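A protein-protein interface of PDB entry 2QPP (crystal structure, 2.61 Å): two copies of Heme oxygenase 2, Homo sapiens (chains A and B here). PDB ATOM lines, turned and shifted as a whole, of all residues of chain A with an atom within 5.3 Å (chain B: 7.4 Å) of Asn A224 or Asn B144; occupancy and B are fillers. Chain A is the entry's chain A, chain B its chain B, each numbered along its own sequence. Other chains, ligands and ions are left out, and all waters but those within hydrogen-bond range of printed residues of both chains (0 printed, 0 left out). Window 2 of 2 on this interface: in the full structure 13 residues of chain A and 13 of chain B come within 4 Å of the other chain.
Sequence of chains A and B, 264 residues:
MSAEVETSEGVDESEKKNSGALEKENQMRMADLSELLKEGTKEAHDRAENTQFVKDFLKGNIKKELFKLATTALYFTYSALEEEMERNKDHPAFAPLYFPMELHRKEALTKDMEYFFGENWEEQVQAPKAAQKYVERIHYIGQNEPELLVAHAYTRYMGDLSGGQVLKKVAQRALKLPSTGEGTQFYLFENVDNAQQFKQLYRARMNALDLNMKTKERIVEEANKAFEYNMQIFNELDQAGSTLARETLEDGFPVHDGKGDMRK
Arg A47 touches His B139 (NE to CB, 3.98 Å). CB of Tyr B140 touches NH1 of Arg A47, 3.8 Å away. Asn A224 touches Tyr B140 (O to CE1, 3.6 Å). Asn A224 touches Asn B144. CG of Lys A225 touches OH of Tyr B140, at 3.2 Å. Glu A228 touches Tyr B140.
Of chain B, only Tyr B140 and Asn B144 come within 4 Å of Asn A224. No residue of chain B comes within 4 Å of Ala A223. Of the printed residues of chain B, Glu A228 touches Tyr B140 (3.5 Å). Printed residues of chain B within 4 Å of Arg A47: His B139, Tyr B140 and Gln B143. Of the printed residues of chain A, Glu B145 touches Lys A225. Printed residues of chain A within 4 Å of Tyr B140: Arg A47, Asn A224, Lys A225 and Glu A228. Of the printed residues of chain B, Lys A225 touches Tyr B140 (3.2 Å) and Glu B145 (3.0 Å). Ile B141 touches none of the printed residues of chain A. The nearest residue of chain B that does not touch Asn A224 is Gln B143 (6.7 Å). The nearest printed residue of chain A that does not touch Glu B145 is Glu A228 (6.3 Å).
The side-chain amide oxygen of Gln B143 sits at hydrogen-bond distance from the guanidinium group of Arg A47. The side-chain carboxylate (OE2) of Glu B145 is in salt-bridge range of the side-chain amino group (NZ) of Lys A225.
No position is printed for both chains.
Of the 14 printed residues of chain A, 4 touch a printed residue of chain B. Of the 14 printed residues of chain B, 5 touch a printed residue of chain A. Among the printed residues, 8 pairs touch across the chains. Among the printed residues, Asp or Glu carboxylates within 4 Å of a Lys or Arg side-chain nitrogen of the other chain: Lys A225 with Glu B145 (3.0 Å).
The backbone carbonyl oxygen (O) of Val A220 is in hydrogen-bond range of the side-chain amide nitrogen (ND2) of Asn A224 (3.0 Å). The side-chain carboxylate of Glu B84 sits at hydrogen-bond distance from the side-chain amide nitrogen of Gln B143, 2.9 Å away. The backbone carbonyl oxygen (O) of His B139 lies close to the side-chain amide nitrogen (NE2) of Gln B143 (3.2 Å). The side-chain amide nitrogen (ND2) of Asn B144 is in hydrogen-bond range of the backbone carbonyl oxygen (O) of Tyr B140, at 3.0 Å. The side-chain hydroxyl (OH) of Tyr B140 sits at hydrogen-bond distance from the side-chain carboxylate (OE2) of Glu B145 (2.5 Å). OE1 of Glu B145 is in salt-bridge range of NH2 of Arg B218.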
ATOM      1  N   GLY A  40      25.866  -7.596  -1.146  1.00  0.00           N
ATOM      2  CA  GLY A  40      25.357  -6.363  -1.732  1.00  0.00           C
ATOM      3  C   GLY A  40      25.243  -5.149  -0.826  1.00  0.00           C
ATOM      4  O   GLY A  40      25.260  -4.018  -1.319  1.00  0.00           O
ATOM      5  N   THR A  41      25.131  -5.365   0.486  1.00  0.00           N
ATOM      6  CA  THR A  41      25.012  -4.252   1.442  1.00  0.00           C
ATOM      7  C   THR A  41      26.212  -4.128   2.395  1.00  0.00           C
ATOM      8  O   THR A  41      26.130  -3.437   3.416  1.00  0.00           O
ATOM      9  CB  THR A  41      23.706  -4.325   2.279  1.00  0.00           C
ATOM     10  OG1 THR A  41      23.689  -5.537   3.040  1.00  0.00           O
ATOM     11  CG2 THR A  41      22.462  -4.257   1.393  1.00  0.00           C
ATOM     12  N   ALA A  44      27.497  -0.512   2.827  1.00  0.00           N
ATOM     13  CA  ALA A  44      26.511   0.198   3.640  1.00  0.00           C
ATOM     14  C   ALA A  44      26.597  -0.168   5.131  1.00  0.00           C
ATOM     15  O   ALA A  44      26.468   0.701   5.998  1.00  0.00           O
ATOM     16  CB  ALA A  44      25.106  -0.038   3.106  1.00  0.00           C
ATOM     17  N   ARG A  47      29.600   1.459   6.721  1.00  0.00           N
ATOM     18  CA  ARG A  47      29.238   2.856   6.954  1.00  0.00           C
ATOM     19  C   ARG A  47      28.394   3.033   8.219  1.00  0.00           C
ATOM     20  O   ARG A  47      28.672   3.913   9.031  1.00  0.00           O
ATOM     21  CB  ARG A  47      28.515   3.437   5.739  1.00  0.00           C
ATOM     22  CG  ARG A  47      29.416   4.222   4.803  1.00  0.00           C
ATOM     23  CD  ARG A  47      28.651   4.714   3.587  1.00  0.00           C
ATOM     24  NE  ARG A  47      28.860   3.833   2.441  1.00  0.00           N
ATOM     25  CZ  ARG A  47      27.899   3.275   1.711  1.00  0.00           C
ATOM     26  NH1 ARG A  47      26.616   3.504   1.962  1.00  0.00           N
ATOM     27  NH2 ARG A  47      28.233   2.494   0.702  1.00  0.00           N
ATOM     28  N   ILE A 219      15.697  -5.842  -4.866  1.00  0.00           N
ATOM     29  CA  ILE A 219      15.670  -5.995  -3.410  1.00  0.00           C
ATOM     30  C   ILE A 219      16.983  -5.502  -2.779  1.00  0.00           C
ATOM     31  O   ILE A 219      16.965  -4.812  -1.762  1.00  0.00           O
ATOM     32  CB  ILE A 219      15.360  -7.460  -2.977  1.00  0.00           C
ATOM     33  CG1 ILE A 219      13.933  -7.844  -3.378  1.00  0.00           C
ATOM     34  CG2 ILE A 219      15.538  -7.634  -1.464  1.00  0.00           C
ATOM     35  CD1 ILE A 219      13.664  -9.333  -3.399  1.00  0.00           C
ATOM     36  N   VAL A 220      18.114  -5.843  -3.391  1.00  0.00           N
ATOM     37  CA  VAL A 220      19.419  -5.427  -2.861  1.00  0.00           C
ATOM     38  C   VAL A 220      19.571  -3.897  -2.871  1.00  0.00           C
ATOM     39  O   VAL A 220      20.089  -3.316  -1.916  1.00  0.00           O
ATOM     40  CB  VAL A 220      20.598  -6.158  -3.570  1.00  0.00           C
ATOM     41  CG1 VAL A 220      21.941  -5.665  -3.067  1.00  0.00           C
ATOM     42  CG2 VAL A 220      20.493  -7.668  -3.342  1.00  0.00           C
ATOM     43  N   GLU A 221      19.079  -3.255  -3.927  1.00  0.00           N
ATOM     44  CA  GLU A 221      19.114  -1.793  -4.042  1.00  0.00           C
ATOM     45  C   GLU A 221      18.237  -1.101  -3.000  1.00  0.00           C
ATOM     46  O   GLU A 221      18.645  -0.102  -2.399  1.00  0.00           O
ATOM     47  CB  GLU A 221      18.706  -1.344  -5.446  1.00  0.00           C
ATOM     48  CG  GLU A 221      19.681  -1.771  -6.529  1.00  0.00           C
ATOM     49  CD  GLU A 221      19.230  -1.366  -7.922  1.00  0.00           C
ATOM     50  OE1 GLU A 221      18.684  -0.248  -8.084  1.00  0.00           O
ATOM     51  OE2 GLU A 221      19.433  -2.171  -8.861  1.00  0.00           O
ATOM     52  N   GLU A 222      17.038  -1.632  -2.788  1.00  0.00           N
ATOM     53  CA  GLU A 222      16.145  -1.083  -1.777  1.00  0.00           C
ATOM     54  C   GLU A 222      16.720  -1.280  -0.368  1.00  0.00           C
ATOM     55  O   GLU A 222      16.569  -0.413   0.493  1.00  0.00           O
ATOM     56  CB  GLU A 222      14.738  -1.676  -1.903  1.00  0.00           C
ATOM     57  CG  GLU A 222      13.663  -0.927  -1.117  1.00  0.00           C
ATOM     58  CD  GLU A 222      13.427   0.501  -1.603  1.00  0.00           C
ATOM     59  OE1 GLU A 222      13.626   0.774  -2.814  1.00  0.00           O
ATOM     60  OE2 GLU A 222      13.026   1.352  -0.772  1.00  0.00           O
ATOM     61  N   ALA A 223      17.393  -2.409  -0.149  1.00  0.00           N
ATOM     62  CA  ALA A 223      18.048  -2.682   1.130  1.00  0.00           C
ATOM     63  C   ALA A 223      19.147  -1.664   1.415  1.00  0.00           C
ATOM     64  O   ALA A 223      19.349  -1.268   2.557  1.00  0.00           O
ATOM     65  CB  ALA A 223      18.604  -4.086   1.156  1.00  0.00           C
ATOM     66  N   ASN A 224      19.849  -1.248   0.364  1.00  0.00           N
ATOM     67  CA  ASN A 224      20.851  -0.199   0.467  1.00  0.00           C
ATOM     68  C   ASN A 224      20.236   1.170   0.751  1.00  0.00           C
ATOM     69  O   ASN A 224      20.776   1.927   1.556  1.00  0.00           O
ATOM     70  CB  ASN A 224      21.732  -0.170  -0.785  1.00  0.00           C
ATOM     71  CG  ASN A 224      22.895  -1.154  -0.700  1.00  0.00           C
ATOM     72  OD1 ASN A 224      23.792  -1.008   0.138  1.00  0.00           O
ATOM     73  ND2 ASN A 224      22.879  -2.162  -1.565  1.00  0.00           N
ATOM     74  N   LYS A 225      19.111   1.476   0.100  1.00  0.00           N
ATOM     75  CA  LYS A 225      18.313   2.658   0.440  1.00  0.00           C
ATOM     76  C   LYS A 225      17.918   2.628   1.912  1.00  0.00           C
ATOM     77  O   LYS A 225      18.097   3.610   2.630  1.00  0.00           O
ATOM     78  CB  LYS A 225      17.042   2.739  -0.414  1.00  0.00           C
ATOM     79  CG  LYS A 225      17.186   3.518  -1.700  1.00  0.00           C
ATOM     80  CD  LYS A 225      15.827   3.873  -2.305  1.00  0.00           C
ATOM     81  CE  LYS A 225      15.245   5.165  -1.715  1.00  0.00           C
ATOM     82  NZ  LYS A 225      15.944   6.413  -2.178  1.00  0.00           N
ATOM     83  N   ALA A 226      17.386   1.487   2.349  1.00  0.00           N
ATOM     84  CA  ALA A 226      16.975   1.281   3.735  1.00  0.00           C
ATOM     85  C   ALA A 226      18.071   1.672   4.724  1.00  0.00           C
ATOM     86  O   ALA A 226      17.799   2.398   5.683  1.00  0.00           O
ATOM     87  CB  ALA A 226      16.527  -0.159   3.953  1.00  0.00           C
ATOM     88  N   PHE A 227      19.301   1.209   4.477  1.00  0.00           N
ATOM     89  CA  PHE A 227      20.469   1.573   5.291  1.00  0.00           C
ATOM     90  C   PHE A 227      20.689   3.083   5.307  1.00  0.00           C
ATOM     91  O   PHE A 227      21.003   3.662   6.345  1.00  0.00           O
ATOM     92  CB  PHE A 227      21.737   0.890   4.765  1.00  0.00           C
ATOM     93  CG  PHE A 227      21.996  -0.472   5.355  1.00  0.00           C
ATOM     94  CD1 PHE A 227      21.590  -1.624   4.687  1.00  0.00           C
ATOM     95  CD2 PHE A 227      22.671  -0.606   6.574  1.00  0.00           C
ATOM     96  CE1 PHE A 227      21.834  -2.884   5.229  1.00  0.00           C
ATOM     97  CE2 PHE A 227      22.922  -1.860   7.115  1.00  0.00           C
ATOM     98  CZ  PHE A 227      22.503  -3.000   6.444  1.00  0.00           C
ATOM     99  N   GLU A 228      20.525   3.717   4.153  1.00  0.00           N
ATOM    100  CA  GLU A 228      20.791   5.147   4.044  1.00  0.00           C
ATOM    101  C   GLU A 228      19.743   5.985   4.772  1.00  0.00           C
ATOM    102  O   GLU A 228      20.065   7.041   5.318  1.00  0.00           O
ATOM    103  CB  GLU A 228      20.924   5.572   2.580  1.00  0.00           C
ATOM    104  CG  GLU A 228      21.335   7.021   2.379  1.00  0.00           C
ATOM    105  CD  GLU A 228      22.700   7.350   2.955  1.00  0.00           C
ATOM    106  OE1 GLU A 228      23.471   6.419   3.277  1.00  0.00           O
ATOM    107  OE2 GLU A 228      23.008   8.554   3.084  1.00  0.00           O
ATOM    108  N   GLU B  84      34.172   8.320  -6.356  1.00  0.00           N
ATOM    109  CA  GLU B  84      32.845   7.967  -6.848  1.00  0.00           C
ATOM    110  C   GLU B  84      32.609   8.364  -8.312  1.00  0.00           C
ATOM    111  O   GLU B  84      31.884   7.678  -9.036  1.00  0.00           O
ATOM    112  CB  GLU B  84      31.752   8.538  -5.926  1.00  0.00           C
ATOM    113  CG  GLU B  84      31.722   7.933  -4.500  1.00  0.00           C
ATOM    114  CD  GLU B  84      31.636   6.406  -4.488  1.00  0.00           C
ATOM    115  OE1 GLU B  84      31.004   5.835  -5.403  1.00  0.00           O
ATOM    116  OE2 GLU B  84      32.195   5.772  -3.562  1.00  0.00           O
ATOM    117  N   ARG B  87      34.349   5.844 -10.341  1.00  0.00           N
ATOM    118  CA  ARG B  87      33.512   4.650 -10.371  1.00  0.00           C
ATOM    119  C   ARG B  87      32.484   4.733 -11.486  1.00  0.00           C
ATOM    120  O   ARG B  87      32.223   3.742 -12.165  1.00  0.00           O
ATOM    121  CB  ARG B  87      32.806   4.450  -9.023  1.00  0.00           C
ATOM    122  CG  ARG B  87      32.125   3.078  -8.854  1.00  0.00           C
ATOM    123  CD  ARG B  87      31.275   2.989  -7.580  1.00  0.00           C
ATOM    124  NE  ARG B  87      31.982   3.482  -6.396  1.00  0.00           N
ATOM    125  CZ  ARG B  87      32.882   2.790  -5.696  1.00  0.00           C
ATOM    126  NH1 ARG B  87      33.208   1.552  -6.043  1.00  0.00           N
ATOM    127  NH2 ARG B  87      33.457   3.340  -4.636  1.00  0.00           N
ATOM    128  N   ASN B  88      31.919   5.923 -11.675  1.00  0.00           N
ATOM    129  CA  ASN B  88      30.820   6.129 -12.615  1.00  0.00           C
ATOM    130  C   ASN B  88      31.226   6.870 -13.885  1.00  0.00           C
ATOM    131  O   ASN B  88      30.378   7.455 -14.567  1.00  0.00           O
ATOM    132  CB  ASN B  88      29.672   6.863 -11.919  1.00  0.00           C
ATOM    133  CG  ASN B  88      29.060   6.048 -10.810  1.00  0.00           C
ATOM    134  OD1 ASN B  88      28.314   5.106 -11.069  1.00  0.00           O
ATOM    135  ND2 ASN B  88      29.383   6.390  -9.562  1.00  0.00           N
ATOM    136  N   ILE B 138      28.368  10.866   0.066  1.00  0.00           N
ATOM    137  CA  ILE B 138      28.956  10.799  -1.267  1.00  0.00           C
ATOM    138  C   ILE B 138      29.149   9.348  -1.714  1.00  0.00           C
ATOM    139  O   ILE B 138      28.771   8.989  -2.830  1.00  0.00           O
ATOM    140  CB  ILE B 138      30.277  11.606  -1.355  1.00  0.00           C
ATOM    141  CG1 ILE B 138      29.993  13.103  -1.192  1.00  0.00           C
ATOM    142  CG2 ILE B 138      30.956  11.376  -2.694  1.00  0.00           C
ATOM    143  CD1 ILE B 138      31.208  13.942  -0.818  1.00  0.00           C
ATOM    144  N   HIS B 139      29.714   8.519  -0.837  1.00  0.00           N
ATOM    145  CA  HIS B 139      29.893   7.097  -1.126  1.00  0.00           C
ATOM    146  C   HIS B 139      28.575   6.375  -1.384  1.00  0.00           C
ATOM    147  O   HIS B 139      28.498   5.541  -2.289  1.00  0.00           O
ATOM    148  CB  HIS B 139      30.667   6.393  -0.013  1.00  0.00           C
ATOM    149  CG  HIS B 139      32.111   6.773   0.047  1.00  0.00           C
ATOM    150  ND1 HIS B 139      32.954   6.669  -1.040  1.00  0.00           N
ATOM    151  CD2 HIS B 139      32.865   7.253   1.064  1.00  0.00           C
ATOM    152  CE1 HIS B 139      34.162   7.081  -0.696  1.00  0.00           C
ATOM    153  NE2 HIS B 139      34.137   7.433   0.578  1.00  0.00           N
ATOM    154  N   TYR B 140      27.546   6.683  -0.594  1.00  0.00           N
ATOM    155  CA  TYR B 140      26.234   6.094  -0.834  1.00  0.00           C
ATOM    156  C   TYR B 140      25.741   6.418  -2.247  1.00  0.00           C
ATOM    157  O   TYR B 140      25.385   5.511  -3.010  1.00  0.00           O
ATOM    158  CB  TYR B 140      25.184   6.541   0.195  1.00  0.00           C
ATOM    159  CG  TYR B 140      23.790   6.181  -0.270  1.00  0.00           C
ATOM    160  CD1 TYR B 140      23.325   4.868  -0.181  1.00  0.00           C
ATOM    161  CD2 TYR B 140      22.955   7.139  -0.854  1.00  0.00           C
ATOM    162  CE1 TYR B 140      22.058   4.522  -0.635  1.00  0.00           C
ATOM    163  CE2 TYR B 140      21.681   6.802  -1.310  1.00  0.00           C
ATOM    164  CZ  TYR B 140      21.245   5.493  -1.199  1.00  0.00           C
ATOM    165  OH  TYR B 140      19.995   5.146  -1.645  1.00  0.00           O
ATOM    166  N   ILE B 141      25.724   7.711  -2.577  1.00  0.00           N
ATOM    167  CA  ILE B 141      25.220   8.189  -3.860  1.00  0.00           C
ATOM    168  C   ILE B 141      25.958   7.558  -5.052  1.00  0.00           C
ATOM    169  O   ILE B 141      25.324   7.020  -5.964  1.00  0.00           O
ATOM    170  CB  ILE B 141      25.238   9.741  -3.939  1.00  0.00           C
ATOM    171  CG1 ILE B 141      24.238  10.352  -2.943  1.00  0.00           C
ATOM    172  CG2 ILE B 141      24.980  10.237  -5.376  1.00  0.00           C
ATOM    173  CD1 ILE B 141      22.756   9.992  -3.168  1.00  0.00           C
ATOM    174  N   GLY B 142      27.287   7.604  -5.025  1.00  0.00           N
ATOM    175  CA  GLY B 142      28.101   7.056  -6.106  1.00  0.00           C
ATOM    176  C   GLY B 142      27.937   5.558  -6.305  1.00  0.00           C
ATOM    177  O   GLY B 142      28.050   5.063  -7.432  1.00  0.00           O
ATOM    178  N   GLN B 143      27.655   4.843  -5.216  1.00  0.00           N
ATOM    179  CA  GLN B 143      27.544   3.383  -5.251  1.00  0.00           C
ATOM    180  C   GLN B 143      26.134   2.862  -5.544  1.00  0.00           C
ATOM    181  O   GLN B 143      25.979   1.755  -6.069  1.00  0.00           O
ATOM    182  CB  GLN B 143      28.076   2.773  -3.945  1.00  0.00           C
ATOM    183  CG  GLN B 143      29.592   2.855  -3.807  1.00  0.00           C
ATOM    184  CD  GLN B 143      30.079   2.782  -2.368  1.00  0.00           C
ATOM    185  OE1 GLN B 143      29.607   1.975  -1.575  1.00  0.00           O
ATOM    186  NE2 GLN B 143      31.045   3.621  -2.036  1.00  0.00           N
ATOM    187  N   ASN B 144      25.114   3.656  -5.215  1.00  0.00           N
ATOM    188  CA  ASN B 144      23.722   3.183  -5.249  1.00  0.00           C
ATOM    189  C   ASN B 144      22.746   4.027  -6.076  1.00  0.00           C
ATOM    190  O   ASN B 144      21.794   3.494  -6.651  1.00  0.00           O
ATOM    191  CB  ASN B 144      23.197   3.031  -3.826  1.00  0.00           C
ATOM    192  CG  ASN B 144      24.049   2.095  -2.996  1.00  0.00           C
ATOM    193  OD1 ASN B 144      23.905   0.877  -3.070  1.00  0.00           O
ATOM    194  ND2 ASN B 144      24.954   2.660  -2.206  1.00  0.00           N
ATOM    195  N   GLU B 145      22.975   5.339  -6.119  1.00  0.00           N
ATOM    196  CA  GLU B 145      22.133   6.247  -6.892  1.00  0.00           C
ATOM    197  C   GLU B 145      23.011   7.222  -7.683  1.00  0.00           C
ATOM    198  O   GLU B 145      22.995   8.425  -7.430  1.00  0.00           O
ATOM    199  CB  GLU B 145      21.145   6.992  -5.980  1.00  0.00           C
ATOM    200  CG  GLU B 145      20.284   6.089  -5.092  1.00  0.00           C
ATOM    201  CD  GLU B 145      19.072   6.793  -4.495  1.00  0.00           C
ATOM    202  OE1 GLU B 145      18.458   7.637  -5.185  1.00  0.00           O
ATOM    203  OE2 GLU B 145      18.710   6.484  -3.339  1.00  0.00           O
ATOM    204  N   PRO B 146      23.780   6.703  -8.658  1.00  0.00           N
ATOM    205  CA  PRO B 146      24.775   7.515  -9.370  1.00  0.00           C
ATOM    206  C   PRO B 146      24.180   8.616 -10.264  1.00  0.00           C
ATOM    207  O   PRO B 146      24.894   9.542 -10.662  1.00  0.00           O
ATOM    208  CB  PRO B 146      25.509   6.481 -10.223  1.00  0.00           C
ATOM    209  CG  PRO B 146      24.492   5.398 -10.445  1.00  0.00           C
ATOM    210  CD  PRO B 146      23.743   5.316  -9.162  1.00  0.00           C
ATOM    211  N   GLU B 147      22.892   8.510 -10.580  1.00  0.00           N
ATOM    212  CA  GLU B 147      22.202   9.559 -11.334  1.00  0.00           C
ATOM    213  C   GLU B 147      22.062  10.850 -10.520  1.00  0.00           C
ATOM    214  O   GLU B 147      21.746  11.903 -11.074  1.00  0.00           O
ATOM    215  CB  GLU B 147      20.834   9.075 -11.851  1.00  0.00           C
ATOM    216  CG  GLU B 147      19.778   8.792 -10.785  1.00  0.00           C
ATOM    217  CD  GLU B 147      19.906   7.417 -10.137  1.00  0.00           C
ATOM    218  OE1 GLU B 147      20.868   6.675 -10.444  1.00  0.00           O
ATOM    219  OE2 GLU B 147      19.032   7.078  -9.308  1.00  0.00           O
ATOM    220  N   ARG B 218      14.735  15.240  -7.662  1.00  0.00           N
ATOM    221  CA  ARG B 218      15.572  14.539  -6.697  1.00  0.00           C
ATOM    222  C   ARG B 218      16.994  15.110  -6.698  1.00  0.00           C
ATOM    223  O   ARG B 218      17.560  15.359  -5.636  1.00  0.00           O
ATOM    224  CB  ARG B 218      15.549  13.023  -6.960  1.00  0.00           C
ATOM    225  CG  ARG B 218      14.321  12.310  -6.354  1.00  0.00           C
ATOM    226  CD  ARG B 218      14.138  10.856  -6.828  1.00  0.00           C
ATOM    227  NE  ARG B 218      15.344  10.032  -6.684  1.00  0.00           N
ATOM    228  CZ  ARG B 218      15.973   9.425  -7.693  1.00  0.00           C
ATOM    229  NH1 ARG B 218      15.514   9.525  -8.936  1.00  0.00           N
ATOM    230  NH2 ARG B 218      17.064   8.704  -7.460  1.00  0.00           N
